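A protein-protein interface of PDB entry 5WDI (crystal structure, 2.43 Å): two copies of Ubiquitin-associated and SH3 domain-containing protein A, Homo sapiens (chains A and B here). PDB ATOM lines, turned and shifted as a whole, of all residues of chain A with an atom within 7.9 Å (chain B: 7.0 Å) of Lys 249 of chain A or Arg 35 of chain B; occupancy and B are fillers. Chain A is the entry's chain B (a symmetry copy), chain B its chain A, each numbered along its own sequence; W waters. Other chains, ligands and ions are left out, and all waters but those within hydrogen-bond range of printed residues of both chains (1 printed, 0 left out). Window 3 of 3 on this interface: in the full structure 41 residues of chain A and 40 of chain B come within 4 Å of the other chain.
OG1 of Thr 250 of chain A sits at hydrogen-bond distance from OD2 of Asp 37 of chain B, 2.7 Å away.
OD2 of Asp 37 of chain B is in hydrogen-bond range of OG1 of Thr 252 of chain A, 2.7 Å away.
The backbone NH of Leu 38 of chain B sits at hydrogen-bond distance from the backbone carbonyl oxygen of Thr 250 of chain A, 2.7 Å away.
O of Thr 252 of chain A lies within hydrogen-bond range of ND2 of Asn 39 of chain B, 2.8 Å away.
NH2 of Arg 35 of chain B is in hydrogen-bond range of O of Leu 38 of chain B, 2.8 Å away.
NE of Arg 35 of chain B lies within hydrogen-bond range of O of Phe 40 of chain B.
The guanidinium group (NE) of Arg 35 of chain B lies close to the backbone carbonyl oxygen (O) of Pro 41 of chain B (3.5 Å).
The backbone carbonyl oxygen (O) of Leu 38 of chain B sits at hydrogen-bond distance from the side-chain hydroxyl (OG) of Ser 62 of chain B.
The backbone NH of Ser 62 of chain B is in hydrogen-bond range of the backbone carbonyl oxygen of Asn 39 of chain B (2.8 Å).
O of Phe 40 of chain B lies within hydrogen-bond range of OG of Ser 62 of chain B.
Among the printed residues, pairs that only touch across the chains: Ile 70 of chain A with Leu 38 of chain B (3.3 Å), Ile 70 of chain A with Ser 62 of chain B (3.3 Å), Ala 74 of chain A with Leu 38 of chain B (3.6 Å), Gly 228 of chain A with Phe 259 of chain B (3.9 Å), Met 229 of chain A with Phe 259 of chain B (3.4 Å), Lys 249 of chain A with Arg 35 of chain B (3.5 Å), Lys 249 of chain A with Pro 36 of chain B (3.6 Å), Lys 249 of chain A with Leu 38 of chain B (3.3 Å), Thr 250 of chain A with Phe 259 of chain B (3.5 Å), Leu 251 of chain A with Asp 37 of chain B (3.6 Å), Leu 251 of chain A with Leu 38 of chain B (3.97 Å) and Leu 251 of chain A with Asn 39 of chain B (3.8 Å).
Lys 249 of chain A touches just these residues of chain B: Arg 35, Pro 36 and Leu 38.
Of chain A, only Lys 249 (3.5 Å) comes within 4 Å of Arg 35 of chain B.
Pro 36 of chain B touches just one residue of chain A: Lys 249.
Printed residues of chain A within 4 Å of Phe 259 of chain B: Gly 228 (3.9 Å), Met 229 (3.4 Å) and Thr 250 (3.5 Å).
Printed residues of chain B within 4 Å of Gly 228 of chain A: Phe 259.
Printed residues of chain B within 4 Å of Ile 70 of chain A: Leu 38 (3.3 Å) and Ser 62 (3.3 Å).
Of the printed residues of chain B, Leu 251 of chain A touches Asp 37 (3.6 Å), Leu 38 (3.97 Å) and Asn 39 (3.8 Å).
Pro 247 of chain A touches none of the printed residues of chain B.
The nearest residue of chain B that does not touch Lys 249 of chain A is Asp 37 of chain B (4.2 Å).
The nearest residue of chain A that does not touch Arg 35 of chain B is Ile 70 of chain A (4.1 Å).
The nearest printed residue of chain A that does not touch Phe 259 of chain B is Pro 246 of chain A (4.6 Å).
Of the 15 printed residues of chain B, 7 touch a printed residue of chain A.
Hydrophobic or aromatic side chains of chain B within 4 Å of the printed part of chain A: Leu 38 and Phe 259.
Along chain B the printed residues that touch a printed residue of chain A span positions 35 to 259.
Of the 18 printed residues of chain A, 8 touch a printed residue of chain B.
Among the printed residues, 16 pairs touch across the chains.
Among the printed residues, no Asp or Glu carboxylate lies within 4 Å of a Lys or Arg side-chain nitrogen of the other chain.
No position is printed for both chains.
Of the 16 pairs that touch across the chains among the printed residues, none has its exchanged pair printed and touching as well.
Water W1 lies within hydrogen-bond range of the backbone carbonyl oxygen of Ile 70 of chain A (2.9 Å), the side-chain carboxylate of Asp 73 of chain A (3.4 Å) and the guanidinium group of Arg 35 of chain B (3.5 Å).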
ATOM      1  N   ILE A  70       7.184  17.067 -11.188  1.00  0.00           N
ATOM      2  CA  ILE A  70       7.112  18.516 -10.994  1.00  0.00           C
ATOM      3  C   ILE A  70       6.220  19.203 -12.041  1.00  0.00           C
ATOM      4  O   ILE A  70       5.624  20.242 -11.765  1.00  0.00           O
ATOM      5  CB  ILE A  70       8.516  19.167 -10.953  1.00  0.00           C
ATOM      6  CG1 ILE A  70       8.416  20.585 -10.386  1.00  0.00           C
ATOM      7  CG2 ILE A  70       9.176  19.188 -12.327  1.00  0.00           C
ATOM      8  CD1 ILE A  70       9.734  21.152  -9.924  1.00  0.00           C
ATOM      9  N   ALA A  71       6.134  18.617 -13.233  1.00  0.00           N
ATOM     10  CA  ALA A  71       5.206  19.081 -14.262  1.00  0.00           C
ATOM     11  C   ALA A  71       3.763  18.775 -13.879  1.00  0.00           C
ATOM     12  O   ALA A  71       2.884  19.623 -14.020  1.00  0.00           O
ATOM     13  CB  ALA A  71       5.528  18.431 -15.595  1.00  0.00           C
ATOM     14  N   ASP A  73       2.671  18.239 -10.896  1.00  0.00           N
ATOM     15  CA  ASP A  73       2.393  19.009  -9.698  1.00  0.00           C
ATOM     16  C   ASP A  73       1.883  20.400 -10.064  1.00  0.00           C
ATOM     17  O   ASP A  73       0.929  20.886  -9.462  1.00  0.00           O
ATOM     18  CB  ASP A  73       3.659  19.110  -8.843  1.00  0.00           C
ATOM     19  CG  ASP A  73       3.416  19.781  -7.507  1.00  0.00           C
ATOM     20  OD1 ASP A  73       3.486  21.027  -7.440  1.00  0.00           O
ATOM     21  OD2 ASP A  73       3.172  19.053  -6.522  1.00  0.00           O
ATOM     22  N   ALA A  74       2.519  21.022 -11.058  1.00  0.00           N
ATOM     23  CA  ALA A  74       2.144  22.364 -11.524  1.00  0.00           C
ATOM     24  C   ALA A  74       0.809  22.390 -12.279  1.00  0.00           C
ATOM     25  O   ALA A  74       0.110  23.403 -12.266  1.00  0.00           O
ATOM     26  CB  ALA A  74       3.252  22.956 -12.388  1.00  0.00           C
ATOM     27  N   LEU A  75       0.469  21.286 -12.940  1.00  0.00           N
ATOM     28  CA  LEU A  75      -0.830  21.150 -13.600  1.00  0.00           C
ATOM     29  C   LEU A  75      -1.966  21.158 -12.589  1.00  0.00           C
ATOM     30  O   LEU A  75      -3.013  21.770 -12.818  1.00  0.00           O
ATOM     31  CB  LEU A  75      -0.899  19.850 -14.404  1.00  0.00           C
ATOM     32  CG  LEU A  75      -0.095  19.804 -15.698  1.00  0.00           C
ATOM     33  CD1 LEU A  75      -0.005  18.371 -16.199  1.00  0.00           C
ATOM     34  CD2 LEU A  75      -0.720  20.703 -16.756  1.00  0.00           C
ATOM     35  N   ASP A  77      -1.844  22.621  -9.663  1.00  0.00           N
ATOM     36  CA  ASP A  77      -1.946  24.001  -9.174  1.00  0.00           C
ATOM     37  C   ASP A  77      -2.692  24.907 -10.157  1.00  0.00           C
ATOM     38  O   ASP A  77      -3.502  25.734  -9.747  1.00  0.00           O
ATOM     39  CB  ASP A  77      -0.558  24.590  -8.892  1.00  0.00           C
ATOM     40  CG  ASP A  77       0.157  23.893  -7.745  1.00  0.00           C
ATOM     41  OD1 ASP A  77      -0.391  22.910  -7.193  1.00  0.00           O
ATOM     42  OD2 ASP A  77       1.280  24.331  -7.402  1.00  0.00           O
ATOM     43  N   SER A  78      -2.412  24.747 -11.449  1.00  0.00           N
ATOM     44  CA  SER A  78      -3.076  25.531 -12.491  1.00  0.00           C
ATOM     45  C   SER A  78      -4.596  25.326 -12.469  1.00  0.00           C
ATOM     46  O   SER A  78      -5.344  26.163 -12.966  1.00  0.00           O
ATOM     47  CB  SER A  78      -2.519  25.173 -13.870  1.00  0.00           C
ATOM     48  OG  SER A  78      -3.019  23.923 -14.309  1.00  0.00           O
ATOM     49  N   LEU A 227       9.185  17.015 -21.035  1.00  0.00           N
ATOM     50  CA  LEU A 227       7.934  17.568 -20.508  1.00  0.00           C
ATOM     51  C   LEU A 227       7.456  18.832 -21.233  1.00  0.00           C
ATOM     52  O   LEU A 227       6.598  19.561 -20.729  1.00  0.00           O
ATOM     53  CB  LEU A 227       8.011  17.781 -18.982  1.00  0.00           C
ATOM     54  CG  LEU A 227       7.671  16.557 -18.111  1.00  0.00           C
ATOM     55  CD1 LEU A 227       6.199  16.184 -18.220  1.00  0.00           C
ATOM     56  CD2 LEU A 227       8.534  15.350 -18.439  1.00  0.00           C
ATOM     57  N   GLY A 228       7.979  19.067 -22.434  1.00  0.00           N
ATOM     58  CA  GLY A 228       7.544  20.191 -23.255  1.00  0.00           C
ATOM     59  C   GLY A 228       6.101  20.002 -23.669  1.00  0.00           C
ATOM     60  O   GLY A 228       5.642  18.872 -23.841  1.00  0.00           O
ATOM     61  N   MET A 229       5.394  21.116 -23.847  1.00  0.00           N
ATOM     62  CA  MET A 229       3.950  21.087 -24.042  1.00  0.00           C
ATOM     63  C   MET A 229       3.459  21.922 -25.197  1.00  0.00           C
ATOM     64  O   MET A 229       4.062  22.931 -25.551  1.00  0.00           O
ATOM     65  CB  MET A 229       3.253  21.587 -22.793  1.00  0.00           C
ATOM     66  CG  MET A 229       3.535  20.750 -21.573  1.00  0.00           C
ATOM     67  SD  MET A 229       2.528  21.276 -20.190  1.00  0.00           S
ATOM     68  CE  MET A 229       3.189  20.201 -18.911  1.00  0.00           C
ATOM     69  N   ASN A 245      -1.113  29.666 -24.815  1.00  0.00           N
ATOM     70  CA  ASN A 245      -0.042  29.529 -23.837  1.00  0.00           C
ATOM     71  C   ASN A 245      -0.313  28.313 -22.951  1.00  0.00           C
ATOM     72  O   ASN A 245      -1.380  28.225 -22.354  1.00  0.00           O
ATOM     73  CB  ASN A 245       0.034  30.791 -22.979  1.00  0.00           C
ATOM     74  CG  ASN A 245       1.127  30.725 -21.926  1.00  0.00           C
ATOM     75  OD1 ASN A 245       2.153  30.066 -22.106  1.00  0.00           O
ATOM     76  ND2 ASN A 245       0.914  31.422 -20.816  1.00  0.00           N
ATOM     77  N   PRO A 246       0.643  27.367 -22.875  1.00  0.00           N
ATOM     78  CA  PRO A 246       0.483  26.185 -22.017  1.00  0.00           C
ATOM     79  C   PRO A 246       0.119  26.525 -20.572  1.00  0.00           C
ATOM     80  O   PRO A 246       0.507  27.577 -20.073  1.00  0.00           O
ATOM     81  CB  PRO A 246       1.862  25.528 -22.075  1.00  0.00           C
ATOM     82  CG  PRO A 246       2.383  25.896 -23.412  1.00  0.00           C
ATOM     83  CD  PRO A 246       1.869  27.280 -23.689  1.00  0.00           C
ATOM     84  N   PRO A 247      -0.612  25.633 -19.895  1.00  0.00           N
ATOM     85  CA  PRO A 247      -1.136  25.977 -18.574  1.00  0.00           C
ATOM     86  C   PRO A 247      -0.074  26.041 -17.478  1.00  0.00           C
ATOM     87  O   PRO A 247      -0.292  26.715 -16.474  1.00  0.00           O
ATOM     88  CB  PRO A 247      -2.157  24.870 -18.292  1.00  0.00           C
ATOM     89  CG  PRO A 247      -1.743  23.721 -19.136  1.00  0.00           C
ATOM     90  CD  PRO A 247      -0.887  24.234 -20.262  1.00  0.00           C
ATOM     91  N   VAL A 248       1.052  25.351 -17.667  1.00  0.00           N
ATOM     92  CA  VAL A 248       2.184  25.447 -16.738  1.00  0.00           C
ATOM     93  C   VAL A 248       3.432  26.011 -17.409  1.00  0.00           C
ATOM     94  O   VAL A 248       3.556  26.023 -18.638  1.00  0.00           O
ATOM     95  CB  VAL A 248       2.524  24.094 -16.070  1.00  0.00           C
ATOM     96  CG1 VAL A 248       1.290  23.512 -15.400  1.00  0.00           C
ATOM     97  CG2 VAL A 248       3.124  23.103 -17.065  1.00  0.00           C
ATOM     98  N   LYS A 249       4.356  26.472 -16.575  1.00  0.00           N
ATOM     99  CA  LYS A 249       5.588  27.095 -17.041  1.00  0.00           C
ATOM    100  C   LYS A 249       6.606  26.065 -17.525  1.00  0.00           C
ATOM    101  O   LYS A 249       6.441  24.857 -17.319  1.00  0.00           O
ATOM    102  CB  LYS A 249       6.206  27.928 -15.914  1.00  0.00           C
ATOM    103  CG  LYS A 249       5.367  29.124 -15.506  1.00  0.00           C
ATOM    104  CD  LYS A 249       5.571  30.297 -16.456  1.00  0.00           C
ATOM    105  CE  LYS A 249       4.577  31.419 -16.192  1.00  0.00           C
ATOM    106  NZ  LYS A 249       4.702  31.963 -14.810  1.00  0.00           N
ATOM    107  N   THR A 250       7.666  26.570 -18.152  1.00  0.00           N
ATOM    108  CA  THR A 250       8.786  25.751 -18.603  1.00  0.00           C
ATOM    109  C   THR A 250       9.598  25.180 -17.432  1.00  0.00           C
ATOM    110  O   THR A 250       9.451  25.613 -16.291  1.00  0.00           O
ATOM    111  CB  THR A 250       9.729  26.572 -19.505  1.00  0.00           C
ATOM    112  OG1 THR A 250      10.141  27.762 -18.818  1.00  0.00           O
ATOM    113  CG2 THR A 250       9.028  26.959 -20.812  1.00  0.00           C
ATOM    114  N   LEU A 251      10.449  24.201 -17.725  1.00  0.00           N
ATOM    115  CA  LEU A 251      11.319  23.591 -16.728  1.00  0.00           C
ATOM    116  C   LEU A 251      12.743  23.587 -17.248  1.00  0.00           C
ATOM    117  O   LEU A 251      13.088  22.791 -18.114  1.00  0.00           O
ATOM    118  CB  LEU A 251      10.880  22.157 -16.423  1.00  0.00           C
ATOM    119  CG  LEU A 251      11.829  21.342 -15.531  1.00  0.00           C
ATOM    120  CD1 LEU A 251      11.926  21.933 -14.127  1.00  0.00           C
ATOM    121  CD2 LEU A 251      11.379  19.895 -15.464  1.00  0.00           C
ATOM    122  N   THR A 252      13.573  24.467 -16.702  1.00  0.00           N
ATOM    123  CA  THR A 252      14.935  24.642 -17.178  1.00  0.00           C
ATOM    124  C   THR A 252      15.890  24.263 -16.066  1.00  0.00           C
ATOM    125  O   THR A 252      15.883  24.894 -15.010  1.00  0.00           O
ATOM    126  CB  THR A 252      15.199  26.109 -17.577  1.00  0.00           C
ATOM    127  OG1 THR A 252      14.123  26.591 -18.393  1.00  0.00           O
ATOM    128  CG2 THR A 252      16.499  26.234 -18.334  1.00  0.00           C
ATOM    129  N   GLN B  25      14.419  38.125 -11.569  1.00  0.00           N
ATOM    130  CA  GLN B  25      13.534  37.381 -12.463  1.00  0.00           C
ATOM    131  C   GLN B  25      12.347  36.766 -11.727  1.00  0.00           C
ATOM    132  O   GLN B  25      11.332  36.452 -12.344  1.00  0.00           O
ATOM    133  CB  GLN B  25      14.299  36.265 -13.169  1.00  0.00           C
ATOM    134  CG  GLN B  25      15.536  36.739 -13.900  1.00  0.00           C
ATOM    135  CD  GLN B  25      16.297  35.615 -14.565  1.00  0.00           C
ATOM    136  OE1 GLN B  25      15.703  34.700 -15.132  1.00  0.00           O
ATOM    137  NE2 GLN B  25      17.627  35.691 -14.523  1.00  0.00           N
ATOM    138  N   CYS B  26      12.475  36.572 -10.419  1.00  0.00           N
ATOM    139  CA  CYS B  26      11.432  35.915  -9.640  1.00  0.00           C
ATOM    140  C   CYS B  26      10.838  36.828  -8.567  1.00  0.00           C
ATOM    141  O   CYS B  26      10.241  36.339  -7.607  1.00  0.00           O
ATOM    142  CB  CYS B  26      12.001  34.654  -8.990  1.00  0.00           C
ATOM    143  SG  CYS B  26      13.346  34.985  -7.839  1.00  0.00           S
ATOM    144  N   TYR B  33       7.520  37.033  -4.170  1.00  0.00           N
ATOM    145  CA  TYR B  33       8.125  35.943  -4.934  1.00  0.00           C
ATOM    146  C   TYR B  33       7.139  35.290  -5.891  1.00  0.00           C
ATOM    147  O   TYR B  33       5.970  35.126  -5.567  1.00  0.00           O
ATOM    148  CB  TYR B  33       8.697  34.885  -3.976  1.00  0.00           C
ATOM    149  CG  TYR B  33       9.342  33.678  -4.647  1.00  0.00           C
ATOM    150  CD1 TYR B  33      10.599  33.767  -5.242  1.00  0.00           C
ATOM    151  CD2 TYR B  33       8.695  32.444  -4.671  1.00  0.00           C
ATOM    152  CE1 TYR B  33      11.189  32.665  -5.849  1.00  0.00           C
ATOM    153  CE2 TYR B  33       9.279  31.336  -5.270  1.00  0.00           C
ATOM    154  CZ  TYR B  33      10.522  31.448  -5.860  1.00  0.00           C
ATOM    155  OH  TYR B  33      11.092  30.335  -6.449  1.00  0.00           O
ATOM    156  N   TYR B  34       7.628  34.923  -7.073  1.00  0.00           N
ATOM    157  CA  TYR B  34       6.877  34.072  -8.005  1.00  0.00           C
ATOM    158  C   TYR B  34       7.850  33.237  -8.830  1.00  0.00           C
ATOM    159  O   TYR B  34       9.034  33.570  -8.930  1.00  0.00           O
ATOM    160  CB  TYR B  34       5.964  34.903  -8.922  1.00  0.00           C
ATOM    161  CG  TYR B  34       6.680  35.647 -10.023  1.00  0.00           C
ATOM    162  CD1 TYR B  34       7.290  36.878  -9.777  1.00  0.00           C
ATOM    163  CD2 TYR B  34       6.742  35.132 -11.321  1.00  0.00           C
ATOM    164  CE1 TYR B  34       7.950  37.572 -10.788  1.00  0.00           C
ATOM    165  CE2 TYR B  34       7.402  35.816 -12.344  1.00  0.00           C
ATOM    166  CZ  TYR B  34       7.998  37.036 -12.072  1.00  0.00           C
ATOM    167  OH  TYR B  34       8.651  37.719 -13.066  1.00  0.00           O
ATOM    168  N   ARG B  35       7.339  32.161  -9.421  1.00  0.00           N
ATOM    169  CA  ARG B  35       8.155  31.229 -10.196  1.00  0.00           C
ATOM    170  C   ARG B  35       7.971  31.450 -11.697  1.00  0.00           C
ATOM    171  O   ARG B  35       6.952  31.036 -12.248  1.00  0.00           O
ATOM    172  CB  ARG B  35       7.753  29.790  -9.864  1.00  0.00           C
ATOM    173  CG  ARG B  35       7.799  29.445  -8.384  1.00  0.00           C
ATOM    174  CD  ARG B  35       7.111  28.115  -8.129  1.00  0.00           C
ATOM    175  NE  ARG B  35       7.855  26.993  -8.704  1.00  0.00           N
ATOM    176  CZ  ARG B  35       7.353  25.776  -8.901  1.00  0.00           C
ATOM    177  NH1 ARG B  35       6.091  25.497  -8.586  1.00  0.00           N
ATOM    178  NH2 ARG B  35       8.117  24.833  -9.431  1.00  0.00           N
ATOM    179  N   PRO B  36       8.949  32.079 -12.371  1.00  0.00           N
ATOM    180  CA  PRO B  36       8.855  32.219 -13.829  1.00  0.00           C
ATOM    181  C   PRO B  36       9.207  30.935 -14.592  1.00  0.00           C
ATOM    182  O   PRO B  36       9.065  30.881 -15.816  1.00  0.00           O
ATOM    183  CB  PRO B  36       9.883  33.307 -14.134  1.00  0.00           C
ATOM    184  CG  PRO B  36      10.911  33.133 -13.077  1.00  0.00           C
ATOM    185  CD  PRO B  36      10.153  32.741 -11.839  1.00  0.00           C
ATOM    186  N   ASP B  37       9.681  29.924 -13.870  1.00  0.00           N
ATOM    187  CA  ASP B  37      10.066  28.642 -14.445  1.00  0.00           C
ATOM    188  C   ASP B  37       9.978  27.609 -13.326  1.00  0.00           C
ATOM    189  O   ASP B  37      10.243  27.923 -12.163  1.00  0.00           O
ATOM    190  CB  ASP B  37      11.481  28.739 -15.022  1.00  0.00           C
ATOM    191  CG  ASP B  37      11.966  27.440 -15.639  1.00  0.00           C
ATOM    192  OD1 ASP B  37      12.367  26.531 -14.888  1.00  0.00           O
ATOM    193  OD2 ASP B  37      11.986  27.335 -16.881  1.00  0.00           O
ATOM    194  N   LEU B  38       9.604  26.383 -13.672  1.00  0.00           N
ATOM    195  CA  LEU B  38       9.339  25.346 -12.677  1.00  0.00           C
ATOM    196  C   LEU B  38      10.556  24.906 -11.870  1.00  0.00           C
ATOM    197  O   LEU B  38      10.407  24.213 -10.853  1.00  0.00           O
ATOM    198  CB  LEU B  38       8.713  24.122 -13.344  1.00  0.00           C
ATOM    199  CG  LEU B  38       7.333  24.335 -13.965  1.00  0.00           C
ATOM    200  CD1 LEU B  38       6.889  23.045 -14.627  1.00  0.00           C
ATOM    201  CD2 LEU B  38       6.300  24.795 -12.940  1.00  0.00           C
ATOM    202  N   ASN B  39      11.747  25.292 -12.316  1.00  0.00           N
ATOM    203  CA  ASN B  39      12.967  24.956 -11.610  1.00  0.00           C
ATOM    204  C   ASN B  39      13.301  25.935 -10.490  1.00  0.00           C
ATOM    205  O   ASN B  39      14.195  25.686  -9.677  1.00  0.00           O
ATOM    206  CB  ASN B  39      14.142  24.840 -12.577  1.00  0.00           C
ATOM    207  CG  ASN B  39      15.292  24.056 -11.984  1.00  0.00           C
ATOM    208  OD1 ASN B  39      15.079  23.092 -11.242  1.00  0.00           O
ATOM    209  ND2 ASN B  39      16.518  24.473 -12.286  1.00  0.00           N
ATOM    210  N   PHE B  40      12.594  27.056 -10.464  1.00  0.00           N
ATOM    211  CA  PHE B  40      12.558  27.892  -9.284  1.00  0.00           C
ATOM    212  C   PHE B  40      11.782  27.115  -8.231  1.00  0.00           C
ATOM    213  O   PHE B  40      10.824  26.422  -8.569  1.00  0.00           O
ATOM    214  CB  PHE B  40      11.873  29.219  -9.580  1.00  0.00           C
ATOM    215  CG  PHE B  40      12.736  30.178 -10.325  1.00  0.00           C
ATOM    216  CD1 PHE B  40      12.860  30.092 -11.701  1.00  0.00           C
ATOM    217  CD2 PHE B  40      13.437  31.164  -9.652  1.00  0.00           C
ATOM    218  CE1 PHE B  40      13.667  30.967 -12.397  1.00  0.00           C
ATOM    219  CE2 PHE B  40      14.243  32.049 -10.344  1.00  0.00           C
ATOM    220  CZ  PHE B  40      14.356  31.949 -11.721  1.00  0.00           C
ATOM    221  N   PRO B  41      12.200  27.203  -6.958  1.00  0.00           N
ATOM    222  CA  PRO B  41      11.537  26.409  -5.926  1.00  0.00           C
ATOM    223  C   PRO B  41      10.096  26.861  -5.677  1.00  0.00           C
ATOM    224  O   PRO B  41       9.754  28.012  -5.955  1.00  0.00           O
ATOM    225  CB  PRO B  41      12.419  26.630  -4.687  1.00  0.00           C
ATOM    226  CG  PRO B  41      13.113  27.927  -4.931  1.00  0.00           C
ATOM    227  CD  PRO B  41      13.306  28.013  -6.414  1.00  0.00           C
ATOM    228  N   CYS B  42       9.273  25.944  -5.171  1.00  0.00           N
ATOM    229  CA  CYS B  42       7.863  26.212  -4.862  1.00  0.00           C
ATOM    230  C   CYS B  42       7.685  27.451  -4.027  1.00  0.00           C
ATOM    231  O   CYS B  42       6.743  28.206  -4.239  1.00  0.00           O
ATOM    232  CB  CYS B  42       7.242  25.037  -4.108  1.00  0.00           C
ATOM    233  SG  CYS B  42       7.058  23.568  -5.138  1.00  0.00           S
ATOM    234  N   SER B  43       8.590  27.644  -3.073  1.00  0.00           N
ATOM    235  CA  SER B  43       8.533  28.773  -2.158  1.00  0.00           C
ATOM    236  C   SER B  43       9.916  29.134  -1.651  1.00  0.00           C
ATOM    237  O   SER B  43      10.861  28.376  -1.827  1.00  0.00           O
ATOM    238  CB  SER B  43       7.629  28.431  -0.968  1.00  0.00           C
ATOM    239  OG  SER B  43       8.056  27.233  -0.355  1.00  0.00           O
ATOM    240  N   SER B  62      14.615  23.452  -8.012  1.00  0.00           N
ATOM    241  CA  SER B  62      13.806  22.234  -7.973  1.00  0.00           C
ATOM    242  C   SER B  62      14.627  20.993  -8.328  1.00  0.00           C
ATOM    243  O   SER B  62      14.448  19.942  -7.731  1.00  0.00           O
ATOM    244  CB  SER B  62      12.621  22.348  -8.926  1.00  0.00           C
ATOM    245  OG  SER B  62      11.956  23.586  -8.766  1.00  0.00           O
ATOM    246  N   PHE B 259      11.780  26.261 -23.745  1.00  0.00           N
ATOM    247  CA  PHE B 259      11.198  26.325 -25.082  1.00  0.00           C
ATOM    248  C   PHE B 259      10.193  27.470 -25.140  1.00  0.00           C
ATOM    249  O   PHE B 259       9.516  27.768 -24.150  1.00  0.00           O
ATOM    250  CB  PHE B 259      10.529  24.990 -25.462  1.00  0.00           C
ATOM    251  CG  PHE B 259       9.204  24.757 -24.789  1.00  0.00           C
ATOM    252  CD1 PHE B 259       9.142  24.239 -23.501  1.00  0.00           C
ATOM    253  CD2 PHE B 259       8.015  25.064 -25.440  1.00  0.00           C
ATOM    254  CE1 PHE B 259       7.917  24.029 -22.874  1.00  0.00           C
ATOM    255  CE2 PHE B 259       6.790  24.861 -24.820  1.00  0.00           C
ATOM    256  CZ  PHE B 259       6.739  24.345 -23.534  1.00  0.00           C
HETATM  257  O   HOH W   1       5.783  22.206  -9.634  1.00  0.00           O
